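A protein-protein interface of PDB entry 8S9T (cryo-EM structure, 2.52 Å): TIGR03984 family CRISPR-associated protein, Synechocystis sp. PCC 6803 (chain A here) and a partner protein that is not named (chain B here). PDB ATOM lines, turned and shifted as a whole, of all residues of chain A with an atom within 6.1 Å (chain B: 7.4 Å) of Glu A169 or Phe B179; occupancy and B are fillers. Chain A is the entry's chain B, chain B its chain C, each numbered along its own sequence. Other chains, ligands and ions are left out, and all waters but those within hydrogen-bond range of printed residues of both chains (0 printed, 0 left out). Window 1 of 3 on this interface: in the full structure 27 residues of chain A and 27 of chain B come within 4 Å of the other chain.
The side-chain hydroxyl (OG) of Ser A167 sits at hydrogen-bond distance from the side-chain carboxylate (OE2) of Glu A185 (2.6 Å).
NH1 of Arg B178 is in hydrogen-bond range of O of Leu B131 (3.1 Å).
The backbone carbonyl oxygen of Gln A120 sits at hydrogen-bond distance from the backbone NH of Ser A167.
The backbone NH of Ile A118 is in hydrogen-bond range of the backbone carbonyl oxygen of Glu A169 (2.9 Å).
The side-chain hydroxyl (OG) of Ser B196 lies within hydrogen-bond range of the side-chain hydroxyl (OG1) of Thr B211, at 2.8 Å.
The backbone carbonyl oxygen of Pro B194 is in hydrogen-bond range of the side-chain hydroxyl of Ser B210 (3.2 Å).
Glu A169 touches two residues of chain B.
Of chain A, only Gln A120, Tyr A122 and Glu A169 come within 4 Å of Phe B179.
Of the printed residues of chain B, Glu A185 touches Arg B178.
Of the printed residues of chain B, Gln A120 touches Arg B178 (3.7 Å), Phe B179 (3.5 Å) and Thr B211 (3.7 Å).
Of the printed residues of chain B, Val A182 touches Leu B131 and Arg B178.
Printed residues of chain B within 4 Å of Ile A171: Leu B131.
Phe A114 touches none of the printed residues of chain B.
Ala B134 touches none of the printed residues of chain A.
The nearest residue of chain B that does not touch Glu A169 is Leu B131 (6.0 Å).
The nearest residue of chain A that does not touch Phe B179 is Glu A185 (5.3 Å).
Along chain A the printed residues that touch a printed residue of chain B span positions 118 to 185.
Among the printed residues, 14 pairs touch across the chains.
Among the printed residues, Asp or Glu carboxylates within 4 Å of a Lys or Arg side-chain nitrogen of the other chain: Glu A169 with Arg B178 (2.6 Å).
The side-chain carboxylate (OE1) of Glu A169 lies within salt-bridge range of the guanidinium group (NH2) of Arg B178.
Among the printed residues, merely in contact across the chains: Ile A118 with Arg B178, Gln A120 with Arg B178, Gln A120 with Phe B179, Gln A120 with Thr B211, Tyr A122 with Arg B178, Tyr A122 with Phe B179, Tyr A122 with Leu B180, Tyr A122 with Pro B194, Glu A169 with Phe B179, Ile A171 with Leu B131, Val A182 with Leu B131, Val A182 with Arg B178 and Glu A185 with Arg B178.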
ATOM      1  N   PHE A 114     -17.226  30.272  18.288  1.00  0.00           N
ATOM      2  CA  PHE A 114     -17.813  29.300  17.382  1.00  0.00           C
ATOM      3  C   PHE A 114     -17.848  29.879  15.978  1.00  0.00           C
ATOM      4  O   PHE A 114     -18.021  31.085  15.793  1.00  0.00           O
ATOM      5  CB  PHE A 114     -19.194  28.822  17.894  1.00  0.00           C
ATOM      6  CG  PHE A 114     -20.266  29.871  17.895  1.00  0.00           C
ATOM      7  CD1 PHE A 114     -21.060  30.083  16.789  1.00  0.00           C
ATOM      8  CD2 PHE A 114     -20.460  30.660  19.010  1.00  0.00           C
ATOM      9  CE1 PHE A 114     -22.035  31.037  16.807  1.00  0.00           C
ATOM     10  CE2 PHE A 114     -21.425  31.618  19.026  1.00  0.00           C
ATOM     11  CZ  PHE A 114     -22.217  31.806  17.926  1.00  0.00           C
ATOM     12  N   THR A 116     -19.879  29.046  13.304  1.00  0.00           N
ATOM     13  CA  THR A 116     -21.231  29.383  12.895  1.00  0.00           C
ATOM     14  C   THR A 116     -22.200  28.636  13.791  1.00  0.00           C
ATOM     15  O   THR A 116     -21.834  27.674  14.468  1.00  0.00           O
ATOM     16  CB  THR A 116     -21.488  29.051  11.428  1.00  0.00           C
ATOM     17  OG1 THR A 116     -22.737  29.625  11.027  1.00  0.00           O
ATOM     18  CG2 THR A 116     -21.533  27.559  11.219  1.00  0.00           C
ATOM     19  N   ALA A 117     -23.446  29.087  13.779  1.00  0.00           N
ATOM     20  CA  ALA A 117     -24.525  28.374  14.437  1.00  0.00           C
ATOM     21  C   ALA A 117     -25.637  28.096  13.445  1.00  0.00           C
ATOM     22  O   ALA A 117     -25.918  28.919  12.572  1.00  0.00           O
ATOM     23  CB  ALA A 117     -25.068  29.180  15.611  1.00  0.00           C
ATOM     24  N   ILE A 118     -26.247  26.923  13.565  1.00  0.00           N
ATOM     25  CA  ILE A 118     -27.233  26.455  12.604  1.00  0.00           C
ATOM     26  C   ILE A 118     -28.506  26.072  13.345  1.00  0.00           C
ATOM     27  O   ILE A 118     -28.453  25.518  14.446  1.00  0.00           O
ATOM     28  CB  ILE A 118     -26.692  25.282  11.758  1.00  0.00           C
ATOM     29  CG1 ILE A 118     -26.410  24.057  12.611  1.00  0.00           C
ATOM     30  CG2 ILE A 118     -25.422  25.685  11.026  1.00  0.00           C
ATOM     31  CD1 ILE A 118     -26.006  22.877  11.797  1.00  0.00           C
ATOM     32  N   ASP A 119     -29.649  26.389  12.743  1.00  0.00           N
ATOM     33  CA  ASP A 119     -30.949  26.091  13.333  1.00  0.00           C
ATOM     34  C   ASP A 119     -31.232  24.597  13.322  1.00  0.00           C
ATOM     35  O   ASP A 119     -30.932  23.903  12.356  1.00  0.00           O
ATOM     36  CB  ASP A 119     -32.049  26.823  12.576  1.00  0.00           C
ATOM     37  CG  ASP A 119     -31.861  28.314  12.580  1.00  0.00           C
ATOM     38  OD1 ASP A 119     -31.301  28.840  13.562  1.00  0.00           O
ATOM     39  OD2 ASP A 119     -32.268  28.965  11.595  1.00  0.00           O
ATOM     40  N   GLN A 120     -31.835  24.109  14.401  1.00  0.00           N
ATOM     41  CA  GLN A 120     -32.321  22.742  14.473  1.00  0.00           C
ATOM     42  C   GLN A 120     -33.722  22.725  15.067  1.00  0.00           C
ATOM     43  O   GLN A 120     -34.131  23.649  15.766  1.00  0.00           O
ATOM     44  CB  GLN A 120     -31.377  21.864  15.303  1.00  0.00           C
ATOM     45  CG  GLN A 120     -29.980  21.708  14.727  1.00  0.00           C
ATOM     46  CD  GLN A 120     -29.938  21.156  13.306  1.00  0.00           C
ATOM     47  OE1 GLN A 120     -30.894  20.564  12.817  1.00  0.00           O
ATOM     48  NE2 GLN A 120     -28.821  21.366  12.638  1.00  0.00           N
ATOM     49  N   TYR A 122     -36.732  20.065  17.003  1.00  0.00           N
ATOM     50  CA  TYR A 122     -37.235  18.807  17.526  1.00  0.00           C
ATOM     51  C   TYR A 122     -38.751  18.827  17.538  1.00  0.00           C
ATOM     52  O   TYR A 122     -39.357  19.697  18.165  1.00  0.00           O
ATOM     53  CB  TYR A 122     -36.666  18.553  18.917  1.00  0.00           C
ATOM     54  CG  TYR A 122     -35.171  18.549  18.901  1.00  0.00           C
ATOM     55  CD1 TYR A 122     -34.481  17.543  18.254  1.00  0.00           C
ATOM     56  CD2 TYR A 122     -34.450  19.588  19.451  1.00  0.00           C
ATOM     57  CE1 TYR A 122     -33.115  17.526  18.230  1.00  0.00           C
ATOM     58  CE2 TYR A 122     -33.087  19.593  19.409  1.00  0.00           C
ATOM     59  CZ  TYR A 122     -32.421  18.557  18.803  1.00  0.00           C
ATOM     60  OH  TYR A 122     -31.054  18.573  18.741  1.00  0.00           O
ATOM     61  N   SER A 167     -33.876  24.983  18.275  1.00  0.00           N
ATOM     62  CA  SER A 167     -32.586  25.024  18.944  1.00  0.00           C
ATOM     63  C   SER A 167     -31.557  25.567  17.970  1.00  0.00           C
ATOM     64  O   SER A 167     -31.822  25.721  16.778  1.00  0.00           O
ATOM     65  CB  SER A 167     -32.158  23.648  19.461  1.00  0.00           C
ATOM     66  OG  SER A 167     -32.149  22.693  18.423  1.00  0.00           O
ATOM     67  N   GLU A 168     -30.399  25.938  18.497  1.00  0.00           N
ATOM     68  CA  GLU A 168     -29.312  26.431  17.669  1.00  0.00           C
ATOM     69  C   GLU A 168     -28.033  25.712  18.064  1.00  0.00           C
ATOM     70  O   GLU A 168     -27.621  25.772  19.224  1.00  0.00           O
ATOM     71  CB  GLU A 168     -29.177  27.940  17.834  1.00  0.00           C
ATOM     72  CG  GLU A 168     -28.196  28.583  16.921  1.00  0.00           C
ATOM     73  CD  GLU A 168     -28.627  29.975  16.542  1.00  0.00           C
ATOM     74  OE1 GLU A 168     -29.499  30.528  17.240  1.00  0.00           O
ATOM     75  OE2 GLU A 168     -28.109  30.517  15.546  1.00  0.00           O
ATOM     76  N   GLU A 169     -27.395  25.053  17.099  1.00  0.00           N
ATOM     77  CA  GLU A 169     -26.152  24.325  17.321  1.00  0.00           C
ATOM     78  C   GLU A 169     -24.972  25.207  16.941  1.00  0.00           C
ATOM     79  O   GLU A 169     -24.941  25.758  15.841  1.00  0.00           O
ATOM     80  CB  GLU A 169     -26.099  23.038  16.502  1.00  0.00           C
ATOM     81  CG  GLU A 169     -27.069  21.977  16.922  1.00  0.00           C
ATOM     82  CD  GLU A 169     -26.981  20.750  16.052  1.00  0.00           C
ATOM     83  OE1 GLU A 169     -26.978  20.902  14.817  1.00  0.00           O
ATOM     84  OE2 GLU A 169     -26.939  19.631  16.598  1.00  0.00           O
ATOM     85  N   TYR A 170     -24.000  25.311  17.833  1.00  0.00           N
ATOM     86  CA  TYR A 170     -22.825  26.144  17.625  1.00  0.00           C
ATOM     87  C   TYR A 170     -21.659  25.283  17.175  1.00  0.00           C
ATOM     88  O   TYR A 170     -21.315  24.309  17.843  1.00  0.00           O
ATOM     89  CB  TYR A 170     -22.480  26.900  18.903  1.00  0.00           C
ATOM     90  CG  TYR A 170     -23.643  27.713  19.387  1.00  0.00           C
ATOM     91  CD1 TYR A 170     -23.892  28.968  18.867  1.00  0.00           C
ATOM     92  CD2 TYR A 170     -24.512  27.213  20.331  1.00  0.00           C
ATOM     93  CE1 TYR A 170     -24.955  29.708  19.289  1.00  0.00           C
ATOM     94  CE2 TYR A 170     -25.578  27.946  20.758  1.00  0.00           C
ATOM     95  CZ  TYR A 170     -25.795  29.195  20.236  1.00  0.00           C
ATOM     96  OH  TYR A 170     -26.872  29.930  20.663  1.00  0.00           O
ATOM     97  N   ILE A 171     -21.056  25.643  16.047  1.00  0.00           N
ATOM     98  CA  ILE A 171     -20.013  24.849  15.412  1.00  0.00           C
ATOM     99  C   ILE A 171     -18.686  25.534  15.668  1.00  0.00           C
ATOM    100  O   ILE A 171     -18.556  26.742  15.450  1.00  0.00           O
ATOM    101  CB  ILE A 171     -20.256  24.698  13.901  1.00  0.00           C
ATOM    102  CG1 ILE A 171     -21.513  23.882  13.630  1.00  0.00           C
ATOM    103  CG2 ILE A 171     -19.074  24.034  13.231  1.00  0.00           C
ATOM    104  CD1 ILE A 171     -21.988  24.026  12.219  1.00  0.00           C
ATOM    105  N   VAL A 182     -20.062  20.509  16.337  1.00  0.00           N
ATOM    106  CA  VAL A 182     -20.988  21.303  17.136  1.00  0.00           C
ATOM    107  C   VAL A 182     -20.613  21.136  18.605  1.00  0.00           C
ATOM    108  O   VAL A 182     -20.515  20.018  19.117  1.00  0.00           O
ATOM    109  CB  VAL A 182     -22.458  20.942  16.845  1.00  0.00           C
ATOM    110  CG1 VAL A 182     -22.565  20.081  15.603  1.00  0.00           C
ATOM    111  CG2 VAL A 182     -23.183  20.334  18.026  1.00  0.00           C
ATOM    112  N   ILE A 183     -20.265  22.247  19.245  1.00  0.00           N
ATOM    113  CA  ILE A 183     -19.761  22.220  20.608  1.00  0.00           C
ATOM    114  C   ILE A 183     -20.870  22.327  21.640  1.00  0.00           C
ATOM    115  O   ILE A 183     -20.704  21.864  22.771  1.00  0.00           O
ATOM    116  CB  ILE A 183     -18.746  23.345  20.810  1.00  0.00           C
ATOM    117  CG1 ILE A 183     -19.316  24.642  20.239  1.00  0.00           C
ATOM    118  CG2 ILE A 183     -17.439  22.967  20.152  1.00  0.00           C
ATOM    119  CD1 ILE A 183     -18.737  25.889  20.822  1.00  0.00           C
ATOM    120  N   ASP A 184     -21.996  22.931  21.283  1.00  0.00           N
ATOM    121  CA  ASP A 184     -23.132  22.956  22.186  1.00  0.00           C
ATOM    122  C   ASP A 184     -24.391  23.198  21.374  1.00  0.00           C
ATOM    123  O   ASP A 184     -24.338  23.588  20.209  1.00  0.00           O
ATOM    124  CB  ASP A 184     -22.954  24.034  23.254  1.00  0.00           C
ATOM    125  CG  ASP A 184     -23.546  23.637  24.576  1.00  0.00           C
ATOM    126  OD1 ASP A 184     -24.527  22.874  24.579  1.00  0.00           O
ATOM    127  OD2 ASP A 184     -23.024  24.081  25.613  1.00  0.00           O
ATOM    128  N   GLU A 185     -25.529  22.955  22.009  1.00  0.00           N
ATOM    129  CA  GLU A 185     -26.818  23.307  21.445  1.00  0.00           C
ATOM    130  C   GLU A 185     -27.660  24.009  22.495  1.00  0.00           C
ATOM    131  O   GLU A 185     -27.845  23.487  23.596  1.00  0.00           O
ATOM    132  CB  GLU A 185     -27.530  22.059  20.926  1.00  0.00           C
ATOM    133  CG  GLU A 185     -28.843  22.332  20.257  1.00  0.00           C
ATOM    134  CD  GLU A 185     -29.586  21.073  19.926  1.00  0.00           C
ATOM    135  OE1 GLU A 185     -29.542  20.125  20.735  1.00  0.00           O
ATOM    136  OE2 GLU A 185     -30.224  21.030  18.858  1.00  0.00           O
ATOM    137  N   ARG A 186     -28.160  25.190  22.153  1.00  0.00           N
ATOM    138  CA  ARG A 186     -29.020  25.972  23.029  1.00  0.00           C
ATOM    139  C   ARG A 186     -30.460  25.851  22.559  1.00  0.00           C
ATOM    140  O   ARG A 186     -30.753  26.087  21.388  1.00  0.00           O
ATOM    141  CB  ARG A 186     -28.557  27.427  23.035  1.00  0.00           C
ATOM    142  CG  ARG A 186     -29.264  28.355  23.985  1.00  0.00           C
ATOM    143  CD  ARG A 186     -28.582  29.719  23.987  1.00  0.00           C
ATOM    144  NE  ARG A 186     -28.673  30.408  22.706  1.00  0.00           N
ATOM    145  CZ  ARG A 186     -29.632  31.260  22.377  1.00  0.00           C
ATOM    146  NH1 ARG A 186     -30.656  31.447  23.186  1.00  0.00           N
ATOM    147  NH2 ARG A 186     -29.621  31.844  21.193  1.00  0.00           N
ATOM    148  N   LEU B 131     -20.848  18.915   8.570  1.00  0.00           N
ATOM    149  CA  LEU B 131     -21.786  19.177   9.658  1.00  0.00           C
ATOM    150  C   LEU B 131     -23.061  19.835   9.159  1.00  0.00           C
ATOM    151  O   LEU B 131     -24.153  19.552   9.662  1.00  0.00           O
ATOM    152  CB  LEU B 131     -21.140  20.048  10.725  1.00  0.00           C
ATOM    153  CG  LEU B 131     -20.051  19.415  11.575  1.00  0.00           C
ATOM    154  CD1 LEU B 131     -19.363  20.502  12.318  1.00  0.00           C
ATOM    155  CD2 LEU B 131     -20.636  18.419  12.528  1.00  0.00           C
ATOM    156  N   ALA B 134     -24.262  17.205   5.787  1.00  0.00           N
ATOM    157  CA  ALA B 134     -24.334  15.768   6.061  1.00  0.00           C
ATOM    158  C   ALA B 134     -24.384  15.514   7.563  1.00  0.00           C
ATOM    159  O   ALA B 134     -23.449  14.958   8.140  1.00  0.00           O
ATOM    160  CB  ALA B 134     -23.160  15.037   5.416  1.00  0.00           C
ATOM    161  N   PRO B 135     -25.434  15.976   8.240  1.00  0.00           N
ATOM    162  CA  PRO B 135     -25.551  15.723   9.680  1.00  0.00           C
ATOM    163  C   PRO B 135     -25.479  14.236  10.011  1.00  0.00           C
ATOM    164  O   PRO B 135     -26.146  13.408   9.389  1.00  0.00           O
ATOM    165  CB  PRO B 135     -26.920  16.316  10.026  1.00  0.00           C
ATOM    166  CG  PRO B 135     -27.672  16.293   8.765  1.00  0.00           C
ATOM    167  CD  PRO B 135     -26.666  16.578   7.704  1.00  0.00           C
ATOM    168  N   GLY B 136     -24.679  13.910  11.022  1.00  0.00           N
ATOM    169  CA  GLY B 136     -24.431  12.543  11.405  1.00  0.00           C
ATOM    170  C   GLY B 136     -23.261  11.872  10.719  1.00  0.00           C
ATOM    171  O   GLY B 136     -22.910  10.749  11.095  1.00  0.00           O
ATOM    172  N   LEU B 137     -22.680  12.493   9.700  1.00  0.00           N
ATOM    173  CA  LEU B 137     -21.474  11.966   9.083  1.00  0.00           C
ATOM    174  C   LEU B 137     -20.280  12.225   9.987  1.00  0.00           C
ATOM    175  O   LEU B 137     -20.066  13.350  10.441  1.00  0.00           O
ATOM    176  CB  LEU B 137     -21.270  12.595   7.713  1.00  0.00           C
ATOM    177  CG  LEU B 137     -20.156  12.084   6.807  1.00  0.00           C
ATOM    178  CD1 LEU B 137     -20.554  10.841   6.079  1.00  0.00           C
ATOM    179  CD2 LEU B 137     -19.884  13.154   5.820  1.00  0.00           C
ATOM    180  N   ALA B 175     -19.820  12.017  16.570  1.00  0.00           N
ATOM    181  CA  ALA B 175     -21.050  12.624  16.075  1.00  0.00           C
ATOM    182  C   ALA B 175     -22.255  12.341  16.967  1.00  0.00           C
ATOM    183  O   ALA B 175     -23.320  12.920  16.731  1.00  0.00           O
ATOM    184  CB  ALA B 175     -21.342  12.145  14.650  1.00  0.00           C
ATOM    185  N   ASN B 176     -22.126  11.446  17.951  1.00  0.00           N
ATOM    186  CA  ASN B 176     -23.237  11.119  18.840  1.00  0.00           C
ATOM    187  C   ASN B 176     -23.690  12.304  19.676  1.00  0.00           C
ATOM    188  O   ASN B 176     -24.794  12.276  20.224  1.00  0.00           O
ATOM    189  CB  ASN B 176     -22.849   9.977  19.783  1.00  0.00           C
ATOM    190  CG  ASN B 176     -22.804   8.640  19.093  1.00  0.00           C
ATOM    191  OD1 ASN B 176     -23.557   8.389  18.153  1.00  0.00           O
ATOM    192  ND2 ASN B 176     -21.919   7.768  19.555  1.00  0.00           N
ATOM    193  N   GLY B 177     -22.860  13.316  19.820  1.00  0.00           N
ATOM    194  CA  GLY B 177     -23.138  14.382  20.748  1.00  0.00           C
ATOM    195  C   GLY B 177     -24.069  15.485  20.307  1.00  0.00           C
ATOM    196  O   GLY B 177     -24.244  16.435  21.072  1.00  0.00           O
ATOM    197  N   ARG B 178     -24.673  15.446  19.123  1.00  0.00           N
ATOM    198  CA  ARG B 178     -25.364  16.641  18.664  1.00  0.00           C
ATOM    199  C   ARG B 178     -26.888  16.559  18.714  1.00  0.00           C
ATOM    200  O   ARG B 178     -27.494  17.308  19.486  1.00  0.00           O
ATOM    201  CB  ARG B 178     -24.814  17.046  17.284  1.00  0.00           C
ATOM    202  CG  ARG B 178     -25.154  16.234  16.111  1.00  0.00           C
ATOM    203  CD  ARG B 178     -24.434  16.811  14.924  1.00  0.00           C
ATOM    204  NE  ARG B 178     -25.046  18.059  14.497  1.00  0.00           N
ATOM    205  CZ  ARG B 178     -24.999  18.529  13.258  1.00  0.00           C
ATOM    206  NH1 ARG B 178     -24.307  17.893  12.334  1.00  0.00           N
ATOM    207  NH2 ARG B 178     -25.599  19.666  12.960  1.00  0.00           N
ATOM    208  N   PHE B 179     -27.551  15.695  17.949  1.00  0.00           N
ATOM    209  CA  PHE B 179     -29.019  15.678  17.966  1.00  0.00           C
ATOM    210  C   PHE B 179     -29.487  14.853  19.158  1.00  0.00           C
ATOM    211  O   PHE B 179     -29.870  13.690  19.031  1.00  0.00           O
ATOM    212  CB  PHE B 179     -29.578  15.117  16.667  1.00  0.00           C
ATOM    213  CG  PHE B 179     -29.114  15.833  15.441  1.00  0.00           C
ATOM    214  CD1 PHE B 179     -29.554  17.103  15.158  1.00  0.00           C
ATOM    215  CD2 PHE B 179     -28.217  15.234  14.577  1.00  0.00           C
ATOM    216  CE1 PHE B 179     -29.126  17.753  14.038  1.00  0.00           C
ATOM    217  CE2 PHE B 179     -27.783  15.886  13.465  1.00  0.00           C
ATOM    218  CZ  PHE B 179     -28.243  17.147  13.192  1.00  0.00           C
ATOM    219  N   LEU B 180     -29.527  15.474  20.333  1.00  0.00           N
ATOM    220  CA  LEU B 180     -29.827  14.708  21.533  1.00  0.00           C
ATOM    221  C   LEU B 180     -31.297  14.753  21.909  1.00  0.00           C
ATOM    222  O   LEU B 180     -31.939  15.807  21.869  1.00  0.00           O
ATOM    223  CB  LEU B 180     -28.996  15.188  22.721  1.00  0.00           C
ATOM    224  CG  LEU B 180     -27.482  15.028  22.657  1.00  0.00           C
ATOM    225  CD1 LEU B 180     -26.828  15.706  23.827  1.00  0.00           C
ATOM    226  CD2 LEU B 180     -27.155  13.563  22.675  1.00  0.00           C
ATOM    227  N   ARG B 181     -31.806  13.585  22.294  1.00  0.00           N
ATOM    228  CA  ARG B 181     -33.166  13.434  22.787  1.00  0.00           C
ATOM    229  C   ARG B 181     -33.468  14.221  24.050  1.00  0.00           C
ATOM    230  O   ARG B 181     -32.731  14.173  25.037  1.00  0.00           O
ATOM    231  CB  ARG B 181     -33.556  11.976  22.999  1.00  0.00           C
ATOM    232  CG  ARG B 181     -35.086  11.867  23.069  1.00  0.00           C
ATOM    233  CD  ARG B 181     -35.826  11.827  21.746  1.00  0.00           C
ATOM    234  NE  ARG B 181     -36.057  10.484  21.253  1.00  0.00           N
ATOM    235  CZ  ARG B 181     -37.212   9.847  21.380  1.00  0.00           C
ATOM    236  NH1 ARG B 181     -38.235  10.450  21.948  1.00  0.00           N
ATOM    237  NH2 ARG B 181     -37.355   8.616  20.923  1.00  0.00           N
ATOM    238  N   LEU B 182     -34.588  14.927  23.998  1.00  0.00           N
ATOM    239  CA  LEU B 182     -35.131  15.723  25.051  1.00  0.00           C
ATOM    240  C   LEU B 182     -36.414  14.978  25.368  1.00  0.00           C
ATOM    241  O   LEU B 182     -37.107  14.554  24.437  1.00  0.00           O
ATOM    242  CB  LEU B 182     -35.446  17.144  24.579  1.00  0.00           C
ATOM    243  CG  LEU B 182     -34.639  18.341  25.070  1.00  0.00           C
ATOM    244  CD1 LEU B 182     -34.437  18.289  26.559  1.00  0.00           C
ATOM    245  CD2 LEU B 182     -33.318  18.404  24.359  1.00  0.00           C
ATOM    246  N   GLU B 192     -32.862   6.083  15.867  1.00  0.00           N
ATOM    247  CA  GLU B 192     -32.833   6.224  17.310  1.00  0.00           C
ATOM    248  C   GLU B 192     -32.788   7.673  17.763  1.00  0.00           C
ATOM    249  O   GLU B 192     -32.806   7.929  18.967  1.00  0.00           O
ATOM    250  CB  GLU B 192     -31.628   5.463  17.865  1.00  0.00           C
ATOM    251  CG  GLU B 192     -30.318   6.227  17.791  1.00  0.00           C
ATOM    252  CD  GLU B 192     -29.590   6.057  16.467  1.00  0.00           C
ATOM    253  OE1 GLU B 192     -30.234   5.688  15.461  1.00  0.00           O
ATOM    254  OE2 GLU B 192     -28.363   6.290  16.433  1.00  0.00           O
ATOM    255  N   LEU B 193     -32.768   8.611  16.838  1.00  0.00           N
ATOM    256  CA  LEU B 193     -32.688  10.038  17.094  1.00  0.00           C
ATOM    257  C   LEU B 193     -34.064  10.638  17.334  1.00  0.00           C
ATOM    258  O   LEU B 193     -35.084  10.041  16.982  1.00  0.00           O
ATOM    259  CB  LEU B 193     -32.008  10.733  15.924  1.00  0.00           C
ATOM    260  CG  LEU B 193     -30.555  10.368  15.642  1.00  0.00           C
ATOM    261  CD1 LEU B 193     -30.065  11.225  14.526  1.00  0.00           C
ATOM    262  CD2 LEU B 193     -29.685  10.548  16.840  1.00  0.00           C
ATOM    263  N   PRO B 194     -34.133  11.808  17.967  1.00  0.00           N
ATOM    264  CA  PRO B 194     -35.396  12.547  17.990  1.00  0.00           C
ATOM    265  C   PRO B 194     -35.853  12.932  16.589  1.00  0.00           C
ATOM    266  O   PRO B 194     -35.052  13.235  15.704  1.00  0.00           O
ATOM    267  CB  PRO B 194     -35.059  13.780  18.829  1.00  0.00           C
ATOM    268  CG  PRO B 194     -33.626  13.965  18.648  1.00  0.00           C
ATOM    269  CD  PRO B 194     -33.048  12.591  18.574  1.00  0.00           C
ATOM    270  N   SER B 196     -37.416  15.419  13.841  1.00  0.00           N
ATOM    271  CA  SER B 196     -37.081  16.809  13.593  1.00  0.00           C
ATOM    272  C   SER B 196     -38.034  17.398  12.569  1.00  0.00           C
ATOM    273  O   SER B 196     -38.351  18.587  12.619  1.00  0.00           O
ATOM    274  CB  SER B 196     -35.635  16.922  13.143  1.00  0.00           C
ATOM    275  OG  SER B 196     -35.334  18.223  12.688  1.00  0.00           O
ATOM    276  N   SER B 210     -35.833  12.094  11.566  1.00  0.00           N
ATOM    277  CA  SER B 210     -34.721  12.903  12.028  1.00  0.00           C
ATOM    278  C   SER B 210     -34.213  13.841  10.945  1.00  0.00           C
ATOM    279  O   SER B 210     -34.499  13.679   9.763  1.00  0.00           O
ATOM    280  CB  SER B 210     -33.570  12.005  12.464  1.00  0.00           C
ATOM    281  OG  SER B 210     -33.958  11.165  13.515  1.00  0.00           O
ATOM    282  N   THR B 211     -33.458  14.853  11.376  1.00  0.00           N
ATOM    283  CA  THR B 211     -32.691  15.662  10.436  1.00  0.00           C
ATOM    284  C   THR B 211     -31.742  14.791   9.634  1.00  0.00           C
ATOM    285  O   THR B 211     -31.540  15.011   8.439  1.00  0.00           O
ATOM    286  CB  THR B 211     -31.902  16.743  11.172  1.00  0.00           C
ATOM    287  OG1 THR B 211     -32.757  17.455  12.069  1.00  0.00           O
ATOM    288  CG2 THR B 211     -31.297  17.718  10.196  1.00  0.00           C
ATOM    289  N   VAL B 212     -31.114  13.825  10.301  1.00  0.00           N
ATOM    290  CA  VAL B 212     -30.231  12.864   9.651  1.00  0.00           C
ATOM    291  C   VAL B 212     -30.976  12.066   8.588  1.00  0.00           C
ATOM    292  O   VAL B 212     -30.544  11.980   7.435  1.00  0.00           O
ATOM    293  CB  VAL B 212     -29.582  11.961  10.713  1.00  0.00           C
ATOM    294  CG1 VAL B 212     -28.709  10.913  10.087  1.00  0.00           C
ATOM    295  CG2 VAL B 212     -28.763  12.806  11.641  1.00  0.00           C
